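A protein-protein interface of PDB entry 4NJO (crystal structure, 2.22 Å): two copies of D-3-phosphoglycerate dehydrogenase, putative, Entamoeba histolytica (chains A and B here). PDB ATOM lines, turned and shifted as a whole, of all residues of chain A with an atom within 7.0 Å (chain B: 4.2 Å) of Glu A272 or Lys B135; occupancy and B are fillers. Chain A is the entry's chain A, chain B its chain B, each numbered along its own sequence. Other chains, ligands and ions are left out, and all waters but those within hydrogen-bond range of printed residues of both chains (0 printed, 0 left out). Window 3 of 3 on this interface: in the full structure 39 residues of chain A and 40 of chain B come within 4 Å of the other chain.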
ATOM      1  N   ALA A  14     -10.248 -27.600  -7.896  1.00  0.00           N
ATOM      2  CA  ALA A  14     -10.935 -28.457  -8.856  1.00  0.00           C
ATOM      3  C   ALA A  14     -11.503 -29.665  -8.110  1.00  0.00           C
ATOM      4  O   ALA A  14     -10.936 -30.098  -7.100  1.00  0.00           O
ATOM      5  CB  ALA A  14      -9.978 -28.901  -9.952  1.00  0.00           C
ATOM      6  N   GLN A 103       4.669 -27.510  -6.021  1.00  0.00           N
ATOM      7  CA  GLN A 103       3.509 -28.288  -6.456  1.00  0.00           C
ATOM      8  C   GLN A 103       2.723 -27.644  -7.605  1.00  0.00           C
ATOM      9  O   GLN A 103       2.284 -28.338  -8.525  1.00  0.00           O
ATOM     10  CB  GLN A 103       2.583 -28.591  -5.273  1.00  0.00           C
ATOM     11  CG  GLN A 103       3.220 -29.409  -4.152  1.00  0.00           C
ATOM     12  CD  GLN A 103       3.583 -30.834  -4.551  1.00  0.00           C
ATOM     13  OE1 GLN A 103       3.185 -31.327  -5.610  1.00  0.00           O
ATOM     14  NE2 GLN A 103       4.342 -31.506  -3.690  1.00  0.00           N
ATOM     15  N   ASN A 104       2.552 -26.326  -7.554  1.00  0.00           N
ATOM     16  CA  ASN A 104       1.824 -25.619  -8.606  1.00  0.00           C
ATOM     17  C   ASN A 104       2.735 -24.868  -9.582  1.00  0.00           C
ATOM     18  O   ASN A 104       2.287 -23.951 -10.276  1.00  0.00           O
ATOM     19  CB  ASN A 104       0.755 -24.688  -8.003  1.00  0.00           C
ATOM     20  CG  ASN A 104       1.340 -23.602  -7.110  1.00  0.00           C
ATOM     21  OD1 ASN A 104       2.532 -23.299  -7.165  1.00  0.00           O
ATOM     22  ND2 ASN A 104       0.488 -22.999  -6.285  1.00  0.00           N
ATOM     23  N   ASN A 106       4.178 -25.484 -12.491  1.00  0.00           N
ATOM     24  CA  ASN A 106       3.961 -25.508 -13.932  1.00  0.00           C
ATOM     25  C   ASN A 106       2.793 -24.644 -14.384  1.00  0.00           C
ATOM     26  O   ASN A 106       2.853 -24.026 -15.444  1.00  0.00           O
ATOM     27  CB  ASN A 106       3.787 -26.934 -14.456  1.00  0.00           C
ATOM     28  CG  ASN A 106       3.908 -27.006 -15.965  1.00  0.00           C
ATOM     29  OD1 ASN A 106       4.916 -26.581 -16.534  1.00  0.00           O
ATOM     30  ND2 ASN A 106       2.879 -27.526 -16.622  1.00  0.00           N
ATOM     31  N   GLY A 107       1.736 -24.615 -13.576  1.00  0.00           N
ATOM     32  CA  GLY A 107       0.586 -23.761 -13.837  1.00  0.00           C
ATOM     33  C   GLY A 107       1.018 -22.318 -14.001  1.00  0.00           C
ATOM     34  O   GLY A 107       0.609 -21.643 -14.946  1.00  0.00           O
ATOM     35  N   ALA A 268      -2.188 -20.623 -10.474  1.00  0.00           N
ATOM     36  CA  ALA A 268      -2.452 -21.950  -9.914  1.00  0.00           C
ATOM     37  C   ALA A 268      -3.870 -22.460 -10.209  1.00  0.00           C
ATOM     38  O   ALA A 268      -4.302 -23.467  -9.640  1.00  0.00           O
ATOM     39  CB  ALA A 268      -2.182 -21.953  -8.415  1.00  0.00           C
ATOM     40  N   GLU A 269      -4.584 -21.777 -11.103  1.00  0.00           N
ATOM     41  CA  GLU A 269      -5.944 -22.179 -11.475  1.00  0.00           C
ATOM     42  C   GLU A 269      -5.975 -23.193 -12.619  1.00  0.00           C
ATOM     43  O   GLU A 269      -6.532 -22.931 -13.690  1.00  0.00           O
ATOM     44  CB  GLU A 269      -6.808 -20.954 -11.806  1.00  0.00           C
ATOM     45  CG  GLU A 269      -7.365 -20.242 -10.584  1.00  0.00           C
ATOM     46  CD  GLU A 269      -8.425 -21.060  -9.872  1.00  0.00           C
ATOM     47  OE1 GLU A 269      -9.555 -21.162 -10.395  1.00  0.00           O
ATOM     48  OE2 GLU A 269      -8.125 -21.606  -8.792  1.00  0.00           O
ATOM     49  N   THR A 270      -5.359 -24.349 -12.390  1.00  0.00           N
ATOM     50  CA  THR A 270      -5.438 -25.465 -13.327  1.00  0.00           C
ATOM     51  C   THR A 270      -5.816 -26.740 -12.591  1.00  0.00           C
ATOM     52  O   THR A 270      -5.594 -26.860 -11.385  1.00  0.00           O
ATOM     53  CB  THR A 270      -4.118 -25.709 -14.096  1.00  0.00           C
ATOM     54  OG1 THR A 270      -3.061 -25.999 -13.175  1.00  0.00           O
ATOM     55  CG2 THR A 270      -3.740 -24.502 -14.942  1.00  0.00           C
ATOM     56  N   GLU A 271      -6.396 -27.678 -13.336  1.00  0.00           N
ATOM     57  CA  GLU A 271      -6.689 -29.019 -12.851  1.00  0.00           C
ATOM     58  C   GLU A 271      -5.445 -29.635 -12.212  1.00  0.00           C
ATOM     59  O   GLU A 271      -5.469 -30.032 -11.048  1.00  0.00           O
ATOM     60  CB  GLU A 271      -7.173 -29.884 -14.026  1.00  0.00           C
ATOM     61  CG  GLU A 271      -7.234 -31.384 -13.764  1.00  0.00           C
ATOM     62  CD  GLU A 271      -8.542 -31.833 -13.140  1.00  0.00           C
ATOM     63  OE1 GLU A 271      -8.739 -33.059 -12.999  1.00  0.00           O
ATOM     64  OE2 GLU A 271      -9.374 -30.968 -12.794  1.00  0.00           O
ATOM     65  N   GLU A 272      -4.360 -29.671 -12.983  1.00  0.00           N
ATOM     66  CA  GLU A 272      -3.123 -30.359 -12.615  1.00  0.00           C
ATOM     67  C   GLU A 272      -2.473 -29.790 -11.351  1.00  0.00           C
ATOM     68  O   GLU A 272      -2.063 -30.546 -10.466  1.00  0.00           O
ATOM     69  CB  GLU A 272      -2.132 -30.326 -13.786  1.00  0.00           C
ATOM     70  CG  GLU A 272      -2.652 -30.933 -15.091  1.00  0.00           C
ATOM     71  CD  GLU A 272      -3.425 -29.951 -15.965  1.00  0.00           C
ATOM     72  OE1 GLU A 272      -3.823 -28.867 -15.480  1.00  0.00           O
ATOM     73  OE2 GLU A 272      -3.642 -30.265 -17.154  1.00  0.00           O
ATOM     74  N   SER A 273      -2.385 -28.462 -11.276  1.00  0.00           N
ATOM     75  CA  SER A 273      -1.784 -27.786 -10.127  1.00  0.00           C
ATOM     76  C   SER A 273      -2.620 -27.919  -8.855  1.00  0.00           C
ATOM     77  O   SER A 273      -2.068 -28.131  -7.774  1.00  0.00           O
ATOM     78  CB  SER A 273      -1.503 -26.314 -10.438  1.00  0.00           C
ATOM     79  OG  SER A 273      -0.373 -26.190 -11.283  1.00  0.00           O
ATOM     80  N   ASN A 274      -3.941 -27.790  -8.985  1.00  0.00           N
ATOM     81  CA  ASN A 274      -4.859 -28.020  -7.864  1.00  0.00           C
ATOM     82  C   ASN A 274      -4.658 -29.401  -7.245  1.00  0.00           C
ATOM     83  O   ASN A 274      -4.562 -29.532  -6.021  1.00  0.00           O
ATOM     84  CB  ASN A 274      -6.316 -27.857  -8.305  1.00  0.00           C
ATOM     85  CG  ASN A 274      -6.756 -26.404  -8.386  1.00  0.00           C
ATOM     86  OD1 ASN A 274      -7.915 -26.123  -8.693  1.00  0.00           O
ATOM     87  ND2 ASN A 274      -5.840 -25.474  -8.110  1.00  0.00           N
ATOM     88  N   ILE A 275      -4.594 -30.417  -8.106  1.00  0.00           N
ATOM     89  CA  ILE A 275      -4.347 -31.801  -7.701  1.00  0.00           C
ATOM     90  C   ILE A 275      -3.035 -31.920  -6.922  1.00  0.00           C
ATOM     91  O   ILE A 275      -3.023 -32.439  -5.807  1.00  0.00           O
ATOM     92  CB  ILE A 275      -4.371 -32.763  -8.920  1.00  0.00           C
ATOM     93  CG1 ILE A 275      -5.806 -32.925  -9.434  1.00  0.00           C
ATOM     94  CG2 ILE A 275      -3.774 -34.124  -8.568  1.00  0.00           C
ATOM     95  CD1 ILE A 275      -5.917 -33.549 -10.811  1.00  0.00           C
ATOM     96  N   ASN A 276      -1.946 -31.420  -7.506  1.00  0.00           N
ATOM     97  CA  ASN A 276      -0.632 -31.459  -6.863  1.00  0.00           C
ATOM     98  C   ASN A 276      -0.590 -30.718  -5.525  1.00  0.00           C
ATOM     99  O   ASN A 276      -0.145 -31.273  -4.519  1.00  0.00           O
ATOM    100  CB  ASN A 276       0.451 -30.915  -7.799  1.00  0.00           C
ATOM    101  CG  ASN A 276       0.722 -31.825  -8.984  1.00  0.00           C
ATOM    102  OD1 ASN A 276       0.352 -33.002  -8.985  1.00  0.00           O
ATOM    103  ND2 ASN A 276       1.379 -31.281 -10.005  1.00  0.00           N
ATOM    104  N   ALA A 277      -1.064 -29.472  -5.523  1.00  0.00           N
ATOM    105  CA  ALA A 277      -1.044 -28.632  -4.325  1.00  0.00           C
ATOM    106  C   ALA A 277      -1.948 -29.173  -3.219  1.00  0.00           C
ATOM    107  O   ALA A 277      -1.540 -29.243  -2.057  1.00  0.00           O
ATOM    108  CB  ALA A 277      -1.418 -27.198  -4.670  1.00  0.00           C
ATOM    109  N   ARG B 130      -6.181 -25.560 -18.132  1.00  0.00           N
ATOM    110  CA  ARG B 130      -5.371 -26.770 -18.227  1.00  0.00           C
ATOM    111  C   ARG B 130      -3.934 -26.445 -18.609  1.00  0.00           C
ATOM    112  O   ARG B 130      -3.642 -25.355 -19.100  1.00  0.00           O
ATOM    113  CB  ARG B 130      -5.986 -27.772 -19.210  1.00  0.00           C
ATOM    114  CG  ARG B 130      -7.141 -28.572 -18.628  1.00  0.00           C
ATOM    115  CD  ARG B 130      -7.200 -29.971 -19.221  1.00  0.00           C
ATOM    116  NE  ARG B 130      -7.772 -29.975 -20.563  1.00  0.00           N
ATOM    117  CZ  ARG B 130      -7.776 -31.023 -21.385  1.00  0.00           C
ATOM    118  NH1 ARG B 130      -7.232 -32.179 -21.018  1.00  0.00           N
ATOM    119  NH2 ARG B 130      -8.326 -30.911 -22.585  1.00  0.00           N
ATOM    120  N   GLU B 131      -3.040 -27.400 -18.374  1.00  0.00           N
ATOM    121  CA  GLU B 131      -1.632 -27.239 -18.713  1.00  0.00           C
ATOM    122  C   GLU B 131      -1.285 -28.025 -19.973  1.00  0.00           C
ATOM    123  O   GLU B 131      -1.834 -29.100 -20.214  1.00  0.00           O
ATOM    124  CB  GLU B 131      -0.749 -27.673 -17.540  1.00  0.00           C
ATOM    125  CG  GLU B 131      -0.864 -26.770 -16.320  1.00  0.00           C
ATOM    126  CD  GLU B 131      -0.278 -27.378 -15.058  1.00  0.00           C
ATOM    127  OE1 GLU B 131       0.609 -28.255 -15.156  1.00  0.00           O
ATOM    128  OE2 GLU B 131      -0.701 -26.969 -13.955  1.00  0.00           O
ATOM    129  N   LEU B 132      -0.382 -27.472 -20.780  1.00  0.00           N
ATOM    130  CA  LEU B 132       0.082 -28.132 -22.000  1.00  0.00           C
ATOM    131  C   LEU B 132       1.013 -29.306 -21.698  1.00  0.00           C
ATOM    132  O   LEU B 132       1.011 -30.306 -22.418  1.00  0.00           O
ATOM    133  CB  LEU B 132       0.780 -27.134 -22.931  1.00  0.00           C
ATOM    134  CG  LEU B 132      -0.034 -25.978 -23.531  1.00  0.00           C
ATOM    135  CD1 LEU B 132       0.885 -25.074 -24.337  1.00  0.00           C
ATOM    136  CD2 LEU B 132      -1.180 -26.476 -24.401  1.00  0.00           C
ATOM    137  N   LYS B 133       1.805 -29.176 -20.636  1.00  0.00           N
ATOM    138  CA  LYS B 133       2.726 -30.232 -20.206  1.00  0.00           C
ATOM    139  C   LYS B 133       2.006 -31.573 -20.017  1.00  0.00           C
ATOM    140  O   LYS B 133       0.900 -31.620 -19.471  1.00  0.00           O
ATOM    141  CB  LYS B 133       3.435 -29.810 -18.917  1.00  0.00           C
ATOM    142  CG  LYS B 133       4.395 -30.834 -18.330  1.00  0.00           C
ATOM    143  CD  LYS B 133       5.018 -30.318 -17.043  1.00  0.00           C
ATOM    144  CE  LYS B 133       5.555 -31.452 -16.185  1.00  0.00           C
ATOM    145  NZ  LYS B 133       4.451 -32.224 -15.549  1.00  0.00           N
ATOM    146  N   ASP B 134       2.647 -32.645 -20.487  1.00  0.00           N
ATOM    147  CA  ASP B 134       2.136 -34.023 -20.387  1.00  0.00           C
ATOM    148  C   ASP B 134       0.910 -34.302 -21.263  1.00  0.00           C
ATOM    149  O   ASP B 134       0.238 -35.323 -21.096  1.00  0.00           O
ATOM    150  CB  ASP B 134       1.865 -34.427 -18.926  1.00  0.00           C
ATOM    151  CG  ASP B 134       3.117 -34.392 -18.061  1.00  0.00           C
ATOM    152  OD1 ASP B 134       4.229 -34.582 -18.596  1.00  0.00           O
ATOM    153  OD2 ASP B 134       2.988 -34.183 -16.836  1.00  0.00           O
ATOM    154  N   LYS B 135       0.627 -33.398 -22.198  1.00  0.00           N
ATOM    155  CA  LYS B 135      -0.456 -33.604 -23.159  1.00  0.00           C
ATOM    156  C   LYS B 135       0.119 -33.966 -24.523  1.00  0.00           C
ATOM    157  O   LYS B 135       1.311 -33.775 -24.770  1.00  0.00           O
ATOM    158  CB  LYS B 135      -1.346 -32.358 -23.262  1.00  0.00           C
ATOM    159  CG  LYS B 135      -1.871 -31.831 -21.933  1.00  0.00           C
ATOM    160  CD  LYS B 135      -2.872 -32.770 -21.274  1.00  0.00           C
ATOM    161  CE  LYS B 135      -3.404 -32.198 -19.965  1.00  0.00           C
ATOM    162  NZ  LYS B 135      -2.337 -31.963 -18.949  1.00  0.00           N
ATOM    163  N   THR B 136      -0.724 -34.494 -25.405  1.00  0.00           N
ATOM    164  CA  THR B 136      -0.279 -34.853 -26.749  1.00  0.00           C
ATOM    165  C   THR B 136      -0.631 -33.759 -27.755  1.00  0.00           C
ATOM    166  O   THR B 136      -1.781 -33.333 -27.844  1.00  0.00           O
ATOM    167  CB  THR B 136      -0.849 -36.216 -27.201  1.00  0.00           C
ATOM    168  OG1 THR B 136      -0.597 -37.198 -26.188  1.00  0.00           O
ATOM    169  CG2 THR B 136      -0.196 -36.675 -28.504  1.00  0.00           C
ATOM    170  N   LEU B 137       0.381 -33.305 -28.491  1.00  0.00           N
ATOM    171  CA  LEU B 137       0.208 -32.344 -29.574  1.00  0.00           C
ATOM    172  C   LEU B 137       0.327 -33.028 -30.934  1.00  0.00           C
ATOM    173  O   LEU B 137       1.278 -33.775 -31.185  1.00  0.00           O
ATOM    174  CB  LEU B 137       1.234 -31.206 -29.470  1.00  0.00           C
ATOM    175  CG  LEU B 137       1.390 -30.271 -30.684  1.00  0.00           C
ATOM    176  CD1 LEU B 137       0.143 -29.429 -30.925  1.00  0.00           C
ATOM    177  CD2 LEU B 137       2.615 -29.385 -30.537  1.00  0.00           C
ATOM    178  N   MET B 158       5.342 -31.627 -24.048  1.00  0.00           N
ATOM    179  CA  MET B 158       4.238 -32.245 -24.768  1.00  0.00           C
ATOM    180  C   MET B 158       4.728 -33.449 -25.568  1.00  0.00           C
ATOM    181  O   MET B 158       5.867 -33.472 -26.036  1.00  0.00           O
ATOM    182  CB  MET B 158       3.559 -31.240 -25.702  1.00  0.00           C
ATOM    183  CG  MET B 158       3.060 -29.975 -25.019  1.00  0.00           C
ATOM    184  SD  MET B 158       2.032 -28.973 -26.110  1.00  0.00           S
ATOM    185  CE  MET B 158       0.452 -29.804 -25.964  1.00  0.00           C
ATOM    186  N   LYS B 159       3.860 -34.447 -25.702  1.00  0.00           N
ATOM    187  CA  LYS B 159       4.117 -35.605 -26.553  1.00  0.00           C
ATOM    188  C   LYS B 159       3.764 -35.229 -27.986  1.00  0.00           C
ATOM    189  O   LYS B 159       2.722 -34.622 -28.235  1.00  0.00           O
ATOM    190  CB  LYS B 159       3.288 -36.806 -26.086  1.00  0.00           C
ATOM    191  CG  LYS B 159       3.595 -37.246 -24.662  1.00  0.00           C
ATOM    192  CD  LYS B 159       2.340 -37.678 -23.918  1.00  0.00           C
ATOM    193  CE  LYS B 159       2.537 -37.553 -22.414  1.00  0.00           C
ATOM    194  NZ  LYS B 159       1.275 -37.743 -21.647  1.00  0.00           N
ATOM    195  N   GLN B 184      -4.648 -34.322 -27.922  1.00  0.00           N
ATOM    196  CA  GLN B 184      -5.446 -33.375 -27.148  1.00  0.00           C
ATOM    197  C   GLN B 184      -5.370 -31.956 -27.711  1.00  0.00           C
ATOM    198  O   GLN B 184      -6.283 -31.154 -27.503  1.00  0.00           O
ATOM    199  CB  GLN B 184      -5.010 -33.401 -25.683  1.00  0.00           C
ATOM    200  CG  GLN B 184      -5.374 -34.695 -24.966  1.00  0.00           C
ATOM    201  CD  GLN B 184      -4.350 -35.098 -23.926  1.00  0.00           C
ATOM    202  OE1 GLN B 184      -3.170 -35.262 -24.233  1.00  0.00           O
ATOM    203  NE2 GLN B 184      -4.801 -35.272 -22.689  1.00  0.00           N
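OE2 of Glu A272 sits at hydrogen-bond distance from N of Glu B131 (3.2 Å).
The side-chain hydroxyl (OG1) of Thr A270 is in hydrogen-bond range of the side-chain carboxylate (OE2) of Glu B131 (2.7 Å).
N of Gly A107 is in hydrogen-bond range of OE2 of Glu B131 (3.4 Å).
The side-chain carboxylate (OE2) of Glu A272 lies within salt-bridge range of the side-chain amino group (NZ) of Lys B135 (2.8 Å).
ND2 of Asn A106 is in hydrogen-bond range of OE1 of Glu B131 (2.8 Å).
The side-chain hydroxyl of Ser A273 sits at hydrogen-bond distance from the side-chain carboxylate of Glu B131 (2.8 Å).
OD2 of Asp B134 is in salt-bridge range of NZ of Lys B133, at 2.8 Å.
The backbone carbonyl oxygen (O) of Lys B133 sits at hydrogen-bond distance from the side-chain amino group (NZ) of Lys B135, 3.3 Å away.
N of Gly A107 sits at hydrogen-bond distance from OG of Ser A273.
The side-chain amino group of Lys B135 lies within hydrogen-bond range of the backbone carbonyl oxygen of Glu B131, 3.2 Å away.
The side-chain hydroxyl (OG1) of Thr A270 lies close to the backbone NH (N) of Ser A273, at 3.2 Å.
O of Lys B135 lies within hydrogen-bond range of N of Lys B159 (2.8 Å).
Among the printed residues, merely in contact across the chains: Asn A106 with Lys B133 and Glu A272 with Arg B130.
Of chain B, only Arg B130 (3.8 Å), Glu B131 (3.2 Å) and Lys B135 (2.8 Å) come within 4 Å of Glu A272.
Lys B135 touches just one residue of chain A: Glu A272.
Printed residues of chain B within 4 Å of Asn A106: Glu B131 (2.8 Å) and Lys B133 (3.3 Å).
Of the printed residues of chain B, Thr A270 touches Glu B131.
Printed residues of chain A within 4 Å of Lys B133: Asn A106.
Of the printed residues of chain B, Gly A107 touches Glu B131.
Of the printed residues of chain A, Glu B131 touches Asn A106 (2.8 Å), Gly A107 (3.4 Å), Thr A270 (2.7 Å), Glu A272 (3.2 Å) and Ser A273 (2.8 Å).
Leu B132 touches none of the printed residues of chain A.
The nearest printed residue of chain B that does not touch Glu A272 is Lys B133 (5.3 Å).
The nearest printed residue of chain B that does not touch Ser A273 is Arg B130 (7.8 Å).
Along chain A the printed residues that touch a printed residue of chain B span positions 106 to 273.
Of the 11 printed residues of chain B, 4 touch a printed residue of chain A.
No position is printed for both chains.
Of the 8 pairs that touch across the chains among the printed residues, none has its exchanged pair printed and touching as well.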
